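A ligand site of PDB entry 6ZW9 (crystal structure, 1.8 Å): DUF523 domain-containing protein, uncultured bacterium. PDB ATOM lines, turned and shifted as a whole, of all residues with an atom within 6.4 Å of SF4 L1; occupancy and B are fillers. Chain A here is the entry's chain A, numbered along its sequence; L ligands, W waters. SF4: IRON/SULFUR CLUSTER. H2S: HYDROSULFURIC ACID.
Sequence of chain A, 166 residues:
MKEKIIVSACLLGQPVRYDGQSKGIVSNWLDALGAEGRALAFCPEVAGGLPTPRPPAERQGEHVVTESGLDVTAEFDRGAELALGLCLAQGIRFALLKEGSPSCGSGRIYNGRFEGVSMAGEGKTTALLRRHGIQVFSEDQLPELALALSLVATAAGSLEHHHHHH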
ATOM      1  N   VAL A   7      18.262   6.381  21.096  1.00  0.00           N
ATOM      2  CA  VAL A   7      17.565   5.109  21.274  1.00  0.00           C
ATOM      3  C   VAL A   7      16.747   5.143  22.555  1.00  0.00           C
ATOM      4  O   VAL A   7      17.271   5.510  23.603  1.00  0.00           O
ATOM      5  CB  VAL A   7      18.560   3.916  21.361  1.00  0.00           C
ATOM      6  CG1 VAL A   7      17.825   2.571  21.420  1.00  0.00           C
ATOM      7  CG2 VAL A   7      19.586   3.936  20.227  1.00  0.00           C
ATOM      8  N   SER A   8      15.494   4.651  22.511  1.00  0.00           N
ATOM      9  CA  SER A   8      14.653   4.528  23.732  1.00  0.00           C
ATOM     10  C   SER A   8      15.454   3.699  24.767  1.00  0.00           C
ATOM     11  O   SER A   8      15.955   2.616  24.425  1.00  0.00           O
ATOM     12  CB  SER A   8      13.382   3.745  23.404  1.00  0.00           C
ATOM     13  OG  SER A   8      12.437   4.538  22.713  1.00  0.00           O
ATOM     14  N   ALA A   9      15.684   4.257  25.950  1.00  0.00           N
ATOM     15  CA  ALA A   9      16.525   3.594  26.955  1.00  0.00           C
ATOM     16  C   ALA A   9      16.088   2.169  27.297  1.00  0.00           C
ATOM     17  O   ALA A   9      16.938   1.315  27.549  1.00  0.00           O
ATOM     18  CB  ALA A   9      16.635   4.466  28.197  1.00  0.00           C
ATOM     19  N   CYS A  10      14.780   1.905  27.228  1.00  0.00           N
ATOM     20  CA  CYS A  10      14.251   0.563  27.518  1.00  0.00           C
ATOM     21  C   CYS A  10      14.735  -0.472  26.478  1.00  0.00           C
ATOM     22  O   CYS A  10      15.003  -1.610  26.853  1.00  0.00           O
ATOM     23  CB  CYS A  10      12.733   0.578  27.620  1.00  0.00           C
ATOM     24  SG  CYS A  10      11.884   1.162  26.129  1.00  0.00           S
ATOM     25  N   LEU A  11      14.899  -0.059  25.213  1.00  0.00           N
ATOM     26  CA  LEU A  11      15.409  -0.960  24.167  1.00  0.00           C
ATOM     27  C   LEU A  11      16.873  -1.370  24.425  1.00  0.00           C
ATOM     28  O   LEU A  11      17.321  -2.379  23.888  1.00  0.00           O
ATOM     29  CB  LEU A  11      15.284  -0.321  22.792  1.00  0.00           C
ATOM     30  CG  LEU A  11      13.844  -0.081  22.309  1.00  0.00           C
ATOM     31  CD1 LEU A  11      13.829   0.656  20.953  1.00  0.00           C
ATOM     32  CD2 LEU A  11      13.039  -1.410  22.217  1.00  0.00           C
ATOM     33  N   GLN A  14      17.550  -0.831  29.877  1.00  0.00           N
ATOM     34  CA  GLN A  14      17.416  -0.030  31.089  1.00  0.00           C
ATOM     35  C   GLN A  14      16.011  -0.199  31.674  1.00  0.00           C
ATOM     36  O   GLN A  14      15.019  -0.212  30.939  1.00  0.00           O
ATOM     37  CB  GLN A  14      17.745   1.424  30.815  1.00  0.00           C
ATOM     38  CG  GLN A  14      19.159   1.609  30.240  1.00  0.00           C
ATOM     39  CD  GLN A  14      19.597   3.045  30.312  1.00  0.00           C
ATOM     40  OE1 GLN A  14      19.100   3.812  31.129  1.00  0.00           O
ATOM     41  NE2 GLN A  14      20.591   3.425  29.521  1.00  0.00           N
ATOM     42  N   VAL A  16      13.553   1.392  32.803  1.00  0.00           N
ATOM     43  CA  VAL A  16      12.841   2.664  32.904  1.00  0.00           C
ATOM     44  C   VAL A  16      11.385   2.597  32.425  1.00  0.00           C
ATOM     45  O   VAL A  16      10.720   3.634  32.405  1.00  0.00           O
ATOM     46  CB  VAL A  16      13.618   3.740  32.104  1.00  0.00           C
ATOM     47  CG1 VAL A  16      14.933   4.092  32.767  1.00  0.00           C
ATOM     48  CG2 VAL A  16      13.827   3.300  30.648  1.00  0.00           C
ATOM     49  N   ARG A  17      10.888   1.421  32.014  1.00  0.00           N
ATOM     50  CA  ARG A  17       9.502   1.284  31.566  1.00  0.00           C
ATOM     51  C   ARG A  17       8.536   1.639  32.693  1.00  0.00           C
ATOM     52  O   ARG A  17       8.929   1.622  33.863  1.00  0.00           O
ATOM     53  CB  ARG A  17       9.237  -0.146  31.051  1.00  0.00           C
ATOM     54  CG  ARG A  17       9.867  -0.394  29.671  1.00  0.00           C
ATOM     55  CD  ARG A  17       8.990   0.129  28.527  1.00  0.00           C
ATOM     56  NE  ARG A  17       7.772  -0.669  28.361  1.00  0.00           N
ATOM     57  CZ  ARG A  17       6.869  -0.483  27.401  1.00  0.00           C
ATOM     58  NH1 ARG A  17       7.045   0.485  26.503  1.00  0.00           N
ATOM     59  NH2 ARG A  17       5.794  -1.259  27.325  1.00  0.00           N
ATOM     60  N   TYR A  18       7.277   1.955  32.347  1.00  0.00           N
ATOM     61  CA  TYR A  18       6.286   2.336  33.352  1.00  0.00           C
ATOM     62  C   TYR A  18       6.137   1.269  34.463  1.00  0.00           C
ATOM     63  O   TYR A  18       5.798   1.615  35.583  1.00  0.00           O
ATOM     64  CB  TYR A  18       4.930   2.633  32.706  1.00  0.00           C
ATOM     65  CG  TYR A  18       4.217   1.380  32.232  1.00  0.00           C
ATOM     66  CD1 TYR A  18       4.646   0.706  31.101  1.00  0.00           C
ATOM     67  CD2 TYR A  18       3.189   0.829  32.972  1.00  0.00           C
ATOM     68  CE1 TYR A  18       4.042  -0.479  30.692  1.00  0.00           C
ATOM     69  CE2 TYR A  18       2.584  -0.367  32.582  1.00  0.00           C
ATOM     70  CZ  TYR A  18       3.000  -1.002  31.421  1.00  0.00           C
ATOM     71  OH  TYR A  18       2.383  -2.147  30.983  1.00  0.00           O
ATOM     72  N   GLN A  21      10.003  -2.605  34.070  1.00  0.00           N
ATOM     73  CA  GLN A  21      10.636  -3.610  33.184  1.00  0.00           C
ATOM     74  C   GLN A  21      11.589  -2.902  32.178  1.00  0.00           C
ATOM     75  O   GLN A  21      11.705  -1.667  32.143  1.00  0.00           O
ATOM     76  CB  GLN A  21       9.581  -4.397  32.369  1.00  0.00           C
ATOM     77  CG  GLN A  21       8.720  -5.405  33.114  1.00  0.00           C
ATOM     78  CD  GLN A  21       8.079  -6.356  32.143  1.00  0.00           C
ATOM     79  OE1 GLN A  21       8.606  -7.439  31.860  1.00  0.00           O
ATOM     80  NE2 GLN A  21       6.930  -5.992  31.583  1.00  0.00           N
ATOM     81  N   LYS A  23      12.998  -3.408  27.849  1.00  0.00           N
ATOM     82  CA  LYS A  23      12.591  -3.987  26.563  1.00  0.00           C
ATOM     83  C   LYS A  23      13.849  -4.225  25.741  1.00  0.00           C
ATOM     84  O   LYS A  23      13.900  -3.866  24.556  1.00  0.00           O
ATOM     85  CB  LYS A  23      11.647  -3.013  25.833  1.00  0.00           C
ATOM     86  CG  LYS A  23      10.290  -2.872  26.502  1.00  0.00           C
ATOM     87  CD  LYS A  23       9.505  -4.174  26.454  1.00  0.00           C
ATOM     88  CE  LYS A  23       8.071  -4.005  26.899  1.00  0.00           C
ATOM     89  NZ  LYS A  23       7.371  -5.306  27.024  1.00  0.00           N
ATOM     90  N   PHE A  42      17.976   7.356  25.758  1.00  0.00           N
ATOM     91  CA  PHE A  42      17.099   8.447  26.182  1.00  0.00           C
ATOM     92  C   PHE A  42      15.728   7.915  26.507  1.00  0.00           C
ATOM     93  O   PHE A  42      15.186   7.125  25.732  1.00  0.00           O
ATOM     94  CB  PHE A  42      17.015   9.535  25.092  1.00  0.00           C
ATOM     95  CG  PHE A  42      16.256  10.767  25.541  1.00  0.00           C
ATOM     96  CD1 PHE A  42      14.898  10.923  25.244  1.00  0.00           C
ATOM     97  CD2 PHE A  42      16.865  11.721  26.330  1.00  0.00           C
ATOM     98  CE1 PHE A  42      14.187  12.019  25.703  1.00  0.00           C
ATOM     99  CE2 PHE A  42      16.155  12.845  26.785  1.00  0.00           C
ATOM    100  CZ  PHE A  42      14.819  12.987  26.450  1.00  0.00           C
ATOM    101  N   CYS A  43      15.156   8.373  27.630  1.00  0.00           N
ATOM    102  CA  CYS A  43      13.779   7.993  27.967  1.00  0.00           C
ATOM    103  C   CYS A  43      13.007   9.295  28.153  1.00  0.00           C
ATOM    104  O   CYS A  43      13.231  10.021  29.118  1.00  0.00           O
ATOM    105  CB  CYS A  43      13.684   7.140  29.230  1.00  0.00           C
ATOM    106  SG  CYS A  43      11.978   6.902  29.789  1.00  0.00           S
ATOM    107  N   PRO A  44      12.125   9.627  27.213  1.00  0.00           N
ATOM    108  CA  PRO A  44      11.355  10.873  27.320  1.00  0.00           C
ATOM    109  C   PRO A  44      10.534  11.023  28.607  1.00  0.00           C
ATOM    110  O   PRO A  44      10.450  12.129  29.133  1.00  0.00           O
ATOM    111  CB  PRO A  44      10.414  10.793  26.094  1.00  0.00           C
ATOM    112  CG  PRO A  44      11.176   9.917  25.101  1.00  0.00           C
ATOM    113  CD  PRO A  44      11.796   8.872  25.974  1.00  0.00           C
ATOM    114  N   GLU A  45       9.958   9.925  29.127  1.00  0.00           N
ATOM    115  CA  GLU A  45       9.116  10.047  30.311  1.00  0.00           C
ATOM    116  C   GLU A  45       9.926  10.335  31.547  1.00  0.00           C
ATOM    117  O   GLU A  45       9.556  11.226  32.327  1.00  0.00           O
ATOM    118  CB  GLU A  45       8.218   8.821  30.445  1.00  0.00           C
ATOM    119  CG  GLU A  45       7.221   8.885  29.306  1.00  0.00           C
ATOM    120  CD  GLU A  45       6.374   7.659  29.069  1.00  0.00           C
ATOM    121  OE1 GLU A  45       6.202   6.887  30.042  1.00  0.00           O
ATOM    122  OE2 GLU A  45       5.869   7.465  27.937  1.00  0.00           O
ATOM    123  N   VAL A  46      11.061   9.647  31.705  1.00  0.00           N
ATOM    124  CA  VAL A  46      11.942   9.932  32.845  1.00  0.00           C
ATOM    125  C   VAL A  46      12.560  11.327  32.703  1.00  0.00           C
ATOM    126  O   VAL A  46      12.584  12.101  33.681  1.00  0.00           O
ATOM    127  CB  VAL A  46      13.014   8.812  33.018  1.00  0.00           C
ATOM    128  CG1 VAL A  46      14.095   9.238  34.011  1.00  0.00           C
ATOM    129  CG2 VAL A  46      12.356   7.498  33.455  1.00  0.00           C
ATOM    130  N   ARG A  54       5.366   4.068  37.032  1.00  0.00           N
ATOM    131  CA  ARG A  54       4.375   5.120  36.814  1.00  0.00           C
ATOM    132  C   ARG A  54       3.159   4.470  36.147  1.00  0.00           C
ATOM    133  O   ARG A  54       3.271   3.411  35.504  1.00  0.00           O
ATOM    134  CB  ARG A  54       4.957   6.277  35.970  1.00  0.00           C
ATOM    135  CG  ARG A  54       5.539   5.803  34.640  1.00  0.00           C
ATOM    136  CD  ARG A  54       6.285   6.910  33.898  1.00  0.00           C
ATOM    137  NE  ARG A  54       6.958   6.408  32.699  1.00  0.00           N
ATOM    138  CZ  ARG A  54       8.132   5.787  32.696  1.00  0.00           C
ATOM    139  NH1 ARG A  54       8.784   5.574  33.831  1.00  0.00           N
ATOM    140  NH2 ARG A  54       8.652   5.352  31.563  1.00  0.00           N
ATOM    141  N   PHE A  76       5.131  14.680  29.219  1.00  0.00           N
ATOM    142  CA  PHE A  76       5.325  14.048  27.914  1.00  0.00           C
ATOM    143  C   PHE A  76       5.900  15.056  26.922  1.00  0.00           C
ATOM    144  O   PHE A  76       6.828  14.735  26.163  1.00  0.00           O
ATOM    145  CB  PHE A  76       3.999  13.496  27.391  1.00  0.00           C
ATOM    146  CG  PHE A  76       3.770  12.060  27.818  1.00  0.00           C
ATOM    147  CD1 PHE A  76       3.521  11.754  29.151  1.00  0.00           C
ATOM    148  CD2 PHE A  76       3.856  11.033  26.901  1.00  0.00           C
ATOM    149  CE1 PHE A  76       3.363  10.426  29.554  1.00  0.00           C
ATOM    150  CE2 PHE A  76       3.661   9.713  27.301  1.00  0.00           C
ATOM    151  CZ  PHE A  76       3.417   9.412  28.621  1.00  0.00           C
ATOM    152  N   LEU A  97      13.104   4.079  18.369  1.00  0.00           N
ATOM    153  CA  LEU A  97      12.203   4.219  19.514  1.00  0.00           C
ATOM    154  C   LEU A  97      11.252   3.036  19.686  1.00  0.00           C
ATOM    155  O   LEU A  97      10.878   2.401  18.707  1.00  0.00           O
ATOM    156  CB  LEU A  97      11.414   5.535  19.405  1.00  0.00           C
ATOM    157  CG  LEU A  97      12.242   6.831  19.240  1.00  0.00           C
ATOM    158  CD1 LEU A  97      11.309   8.063  19.244  1.00  0.00           C
ATOM    159  CD2 LEU A  97      13.307   6.974  20.345  1.00  0.00           C
ATOM    160  N   LYS A  98      10.838   2.782  20.933  1.00  0.00           N
ATOM    161  CA  LYS A  98       9.970   1.668  21.297  1.00  0.00           C
ATOM    162  C   LYS A  98       8.550   1.771  20.724  1.00  0.00           C
ATOM    163  O   LYS A  98       7.824   2.744  20.980  1.00  0.00           O
ATOM    164  CB  LYS A  98       9.911   1.547  22.832  1.00  0.00           C
ATOM    165  CG  LYS A  98       8.968   0.449  23.336  1.00  0.00           C
ATOM    166  CD  LYS A  98       9.511  -0.956  23.056  1.00  0.00           C
ATOM    167  CE  LYS A  98       8.426  -2.019  23.216  1.00  0.00           C
ATOM    168  NZ  LYS A  98       7.487  -2.053  22.059  1.00  0.00           N
ATOM    169  N   GLU A  99       8.127   0.739  20.002  1.00  0.00           N
ATOM    170  CA  GLU A  99       6.797   0.712  19.394  1.00  0.00           C
ATOM    171  C   GLU A  99       5.645   0.668  20.427  1.00  0.00           C
ATOM    172  O   GLU A  99       5.804   0.127  21.514  1.00  0.00           O
ATOM    173  CB  GLU A  99       6.695  -0.479  18.423  1.00  0.00           C
ATOM    174  CG  GLU A  99       5.455  -0.453  17.531  1.00  0.00           C
ATOM    175  CD  GLU A  99       5.292   0.804  16.693  1.00  0.00           C
ATOM    176  OE1 GLU A  99       4.955   1.877  17.260  1.00  0.00           O
ATOM    177  OE2 GLU A  99       5.501   0.733  15.456  1.00  0.00           O
ATOM    178  N   SER A 101       4.279   2.929  22.361  1.00  0.00           N
ATOM    179  CA  SER A 101       4.329   3.846  23.500  1.00  0.00           C
ATOM    180  C   SER A 101       3.661   5.209  23.214  1.00  0.00           C
ATOM    181  O   SER A 101       3.842   5.770  22.133  1.00  0.00           O
ATOM    182  CB  SER A 101       5.792   4.020  23.927  1.00  0.00           C
ATOM    183  OG  SER A 101       6.078   5.207  24.644  1.00  0.00           O
ATOM    184  N   PRO A 102       3.043   5.825  24.229  1.00  0.00           N
ATOM    185  CA  PRO A 102       2.476   7.181  24.031  1.00  0.00           C
ATOM    186  C   PRO A 102       3.571   8.255  23.846  1.00  0.00           C
ATOM    187  O   PRO A 102       3.233   9.389  23.475  1.00  0.00           O
ATOM    188  CB  PRO A 102       1.662   7.409  25.312  1.00  0.00           C
ATOM    189  CG  PRO A 102       2.343   6.551  26.352  1.00  0.00           C
ATOM    190  CD  PRO A 102       2.789   5.316  25.598  1.00  0.00           C
ATOM    191  N   SER A 103       4.846   7.919  24.109  1.00  0.00           N
ATOM    192  CA  SER A 103       5.985   8.794  23.851  1.00  0.00           C
ATOM    193  C   SER A 103       6.710   8.307  22.581  1.00  0.00           C
ATOM    194  O   SER A 103       6.982   9.106  21.684  1.00  0.00           O
ATOM    195  CB  SER A 103       7.007   8.729  24.991  1.00  0.00           C
ATOM    196  OG  SER A 103       6.611   9.448  26.146  1.00  0.00           O
ATOM    197  N   CYS A 104       7.086   7.026  22.556  1.00  0.00           N
ATOM    198  CA  CYS A 104       8.009   6.441  21.602  1.00  0.00           C
ATOM    199  C   CYS A 104       7.395   5.685  20.404  1.00  0.00           C
ATOM    200  O   CYS A 104       8.118   5.349  19.474  1.00  0.00           O
ATOM    201  CB  CYS A 104       8.979   5.544  22.374  1.00  0.00           C
ATOM    202  SG  CYS A 104      10.018   6.450  23.550  1.00  0.00           S
ATOM    203  N   GLY A 105       6.091   5.421  20.434  1.00  0.00           N
ATOM    204  CA  GLY A 105       5.412   4.706  19.350  1.00  0.00           C
ATOM    205  C   GLY A 105       5.607   5.391  17.999  1.00  0.00           C
ATOM    206  O   GLY A 105       5.698   6.627  17.964  1.00  0.00           O
HETATM  207 FE1  SF4 L   1       8.652   4.237  27.797  1.00  0.00          FE
HETATM  208 FE2  SF4 L   1      10.982   3.146  26.769  1.00  0.00          FE
HETATM  209 FE3  SF4 L   1      11.069   5.536  28.202  1.00  0.00          FE
HETATM  210 FE4  SF4 L   1       9.970   5.454  25.655  1.00  0.00          FE
HETATM  211  S1  SF4 L   1      12.186   5.048  26.272  1.00  0.00           S
HETATM  212  S2  SF4 L   1       9.089   6.525  27.490  1.00  0.00           S
HETATM  213  S3  SF4 L   1       8.934   3.381  25.682  1.00  0.00           S
HETATM  214  S4  SF4 L   1      10.481   3.449  28.998  1.00  0.00           S
HETATM  215  S   H2S L   2       7.070   3.344  29.243  1.00  0.00           S
HETATM  216  O   HOH W   1       5.803   4.870  27.260  1.00  0.00           O
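S of H2S L2 binds FE1 of SF4 L1 (2.3 Å).
A sulfur (S4) of SF4 L1 lies close to the backbone carbonyl oxygen of Val 16.
The backbone carbonyl oxygen (O) of Phe 42 lies close to a sulfur (S1) of SF4 L1 (3.7 Å).
A sulfur (S2) of SF4 L1 lies close to the side-chain carboxylate (OE2) of Glu 45 (3.4 Å).
Pro 44 touches SF4 L1 (CD to S1, 3.9 Å).
Lys 98 touches SF4 L1 (CB to S3, 3.5 Å).
Ser 103 touches SF4 L1 (CB to S2, 3.9 Å).
Hydrophobic or aromatic side chains within 4 Å of SF4 L1: Val 16 and Pro 44.
Within 4 Å of SF4 L1: Ser 8, Ala 9, Cys 10, Val 16, Arg 17, Phe 42, Cys 43, Pro 44, Glu 45, Arg 54, Lys 98, Ser 101, Ser 103 and Cys 104.
The side-chain sulfur (SG) of Cys 10 is bound to an iron atom (FE2) of SF4 L1.
FE3 of SF4 L1 is bound by SG of Cys 43 (2.3 Å).
SG of Cys 104 is bound to FE4 of SF4 L1.
S1 of SF4 L1 lies close to OG of Ser 8 (3.6 Å).
N of Arg 17 lies close to S4 of SF4 L1.
The guanidinium group of Arg 17 sits close to a sulfur (S3) of SF4 L1 (3.6 Å).
The side-chain hydroxyl of Ser 101 lies close to a sulfur (S3) of SF4 L1.
The backbone NH (N) of Ala 9 lies close to a sulfur (S1) of SF4 L1 (3.6 Å).
A sulfur (S4) of SF4 L1 lies close to the guanidinium group (NH2) of Arg 54 (3.7 Å).
The side-chain carboxylate (OE1) of Glu 45 sits close to a sulfur (S) of H2S L2 (3.7 Å).
The guanidinium group (NH2) of Arg 54 lies close to a sulfur (S) of H2S L2 (3.5 Å).
A sulfur (S) of H2S L2 lies close to the backbone NH of Tyr 18, 3.4 Å away.
The backbone NH of Lys 23 is in hydrogen-bond range of the backbone carbonyl oxygen of Cys 10.
The side-chain hydroxyl (OG) of Ser 8 sits close to the side-chain sulfur (SG) of Cys 104, at 3.2 Å.
The backbone NH of Cys 104 is in hydrogen-bond range of the side-chain hydroxyl of Ser 101 (2.9 Å).
OG of Ser 103 sits at hydrogen-bond distance from OE2 of Glu 45 (2.8 Å).
O of Val 16 is in hydrogen-bond range of NH2 of Arg 54, at 2.8 Å.
The backbone NH (N) of Gly 105 lies within hydrogen-bond range of the backbone carbonyl oxygen (O) of Lys 98 (3.2 Å).
N of Ala 9 is in hydrogen-bond range of O of Phe 42, at 2.9 Å.
N of Phe 42 sits at hydrogen-bond distance from O of Val 7 (2.9 Å).
Water W1 lies within hydrogen-bond range of OG of Ser 101 (2.7 Å), OE2 of Glu 45 (2.7 Å) and S2 of SF4 L1 (3.7 Å).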
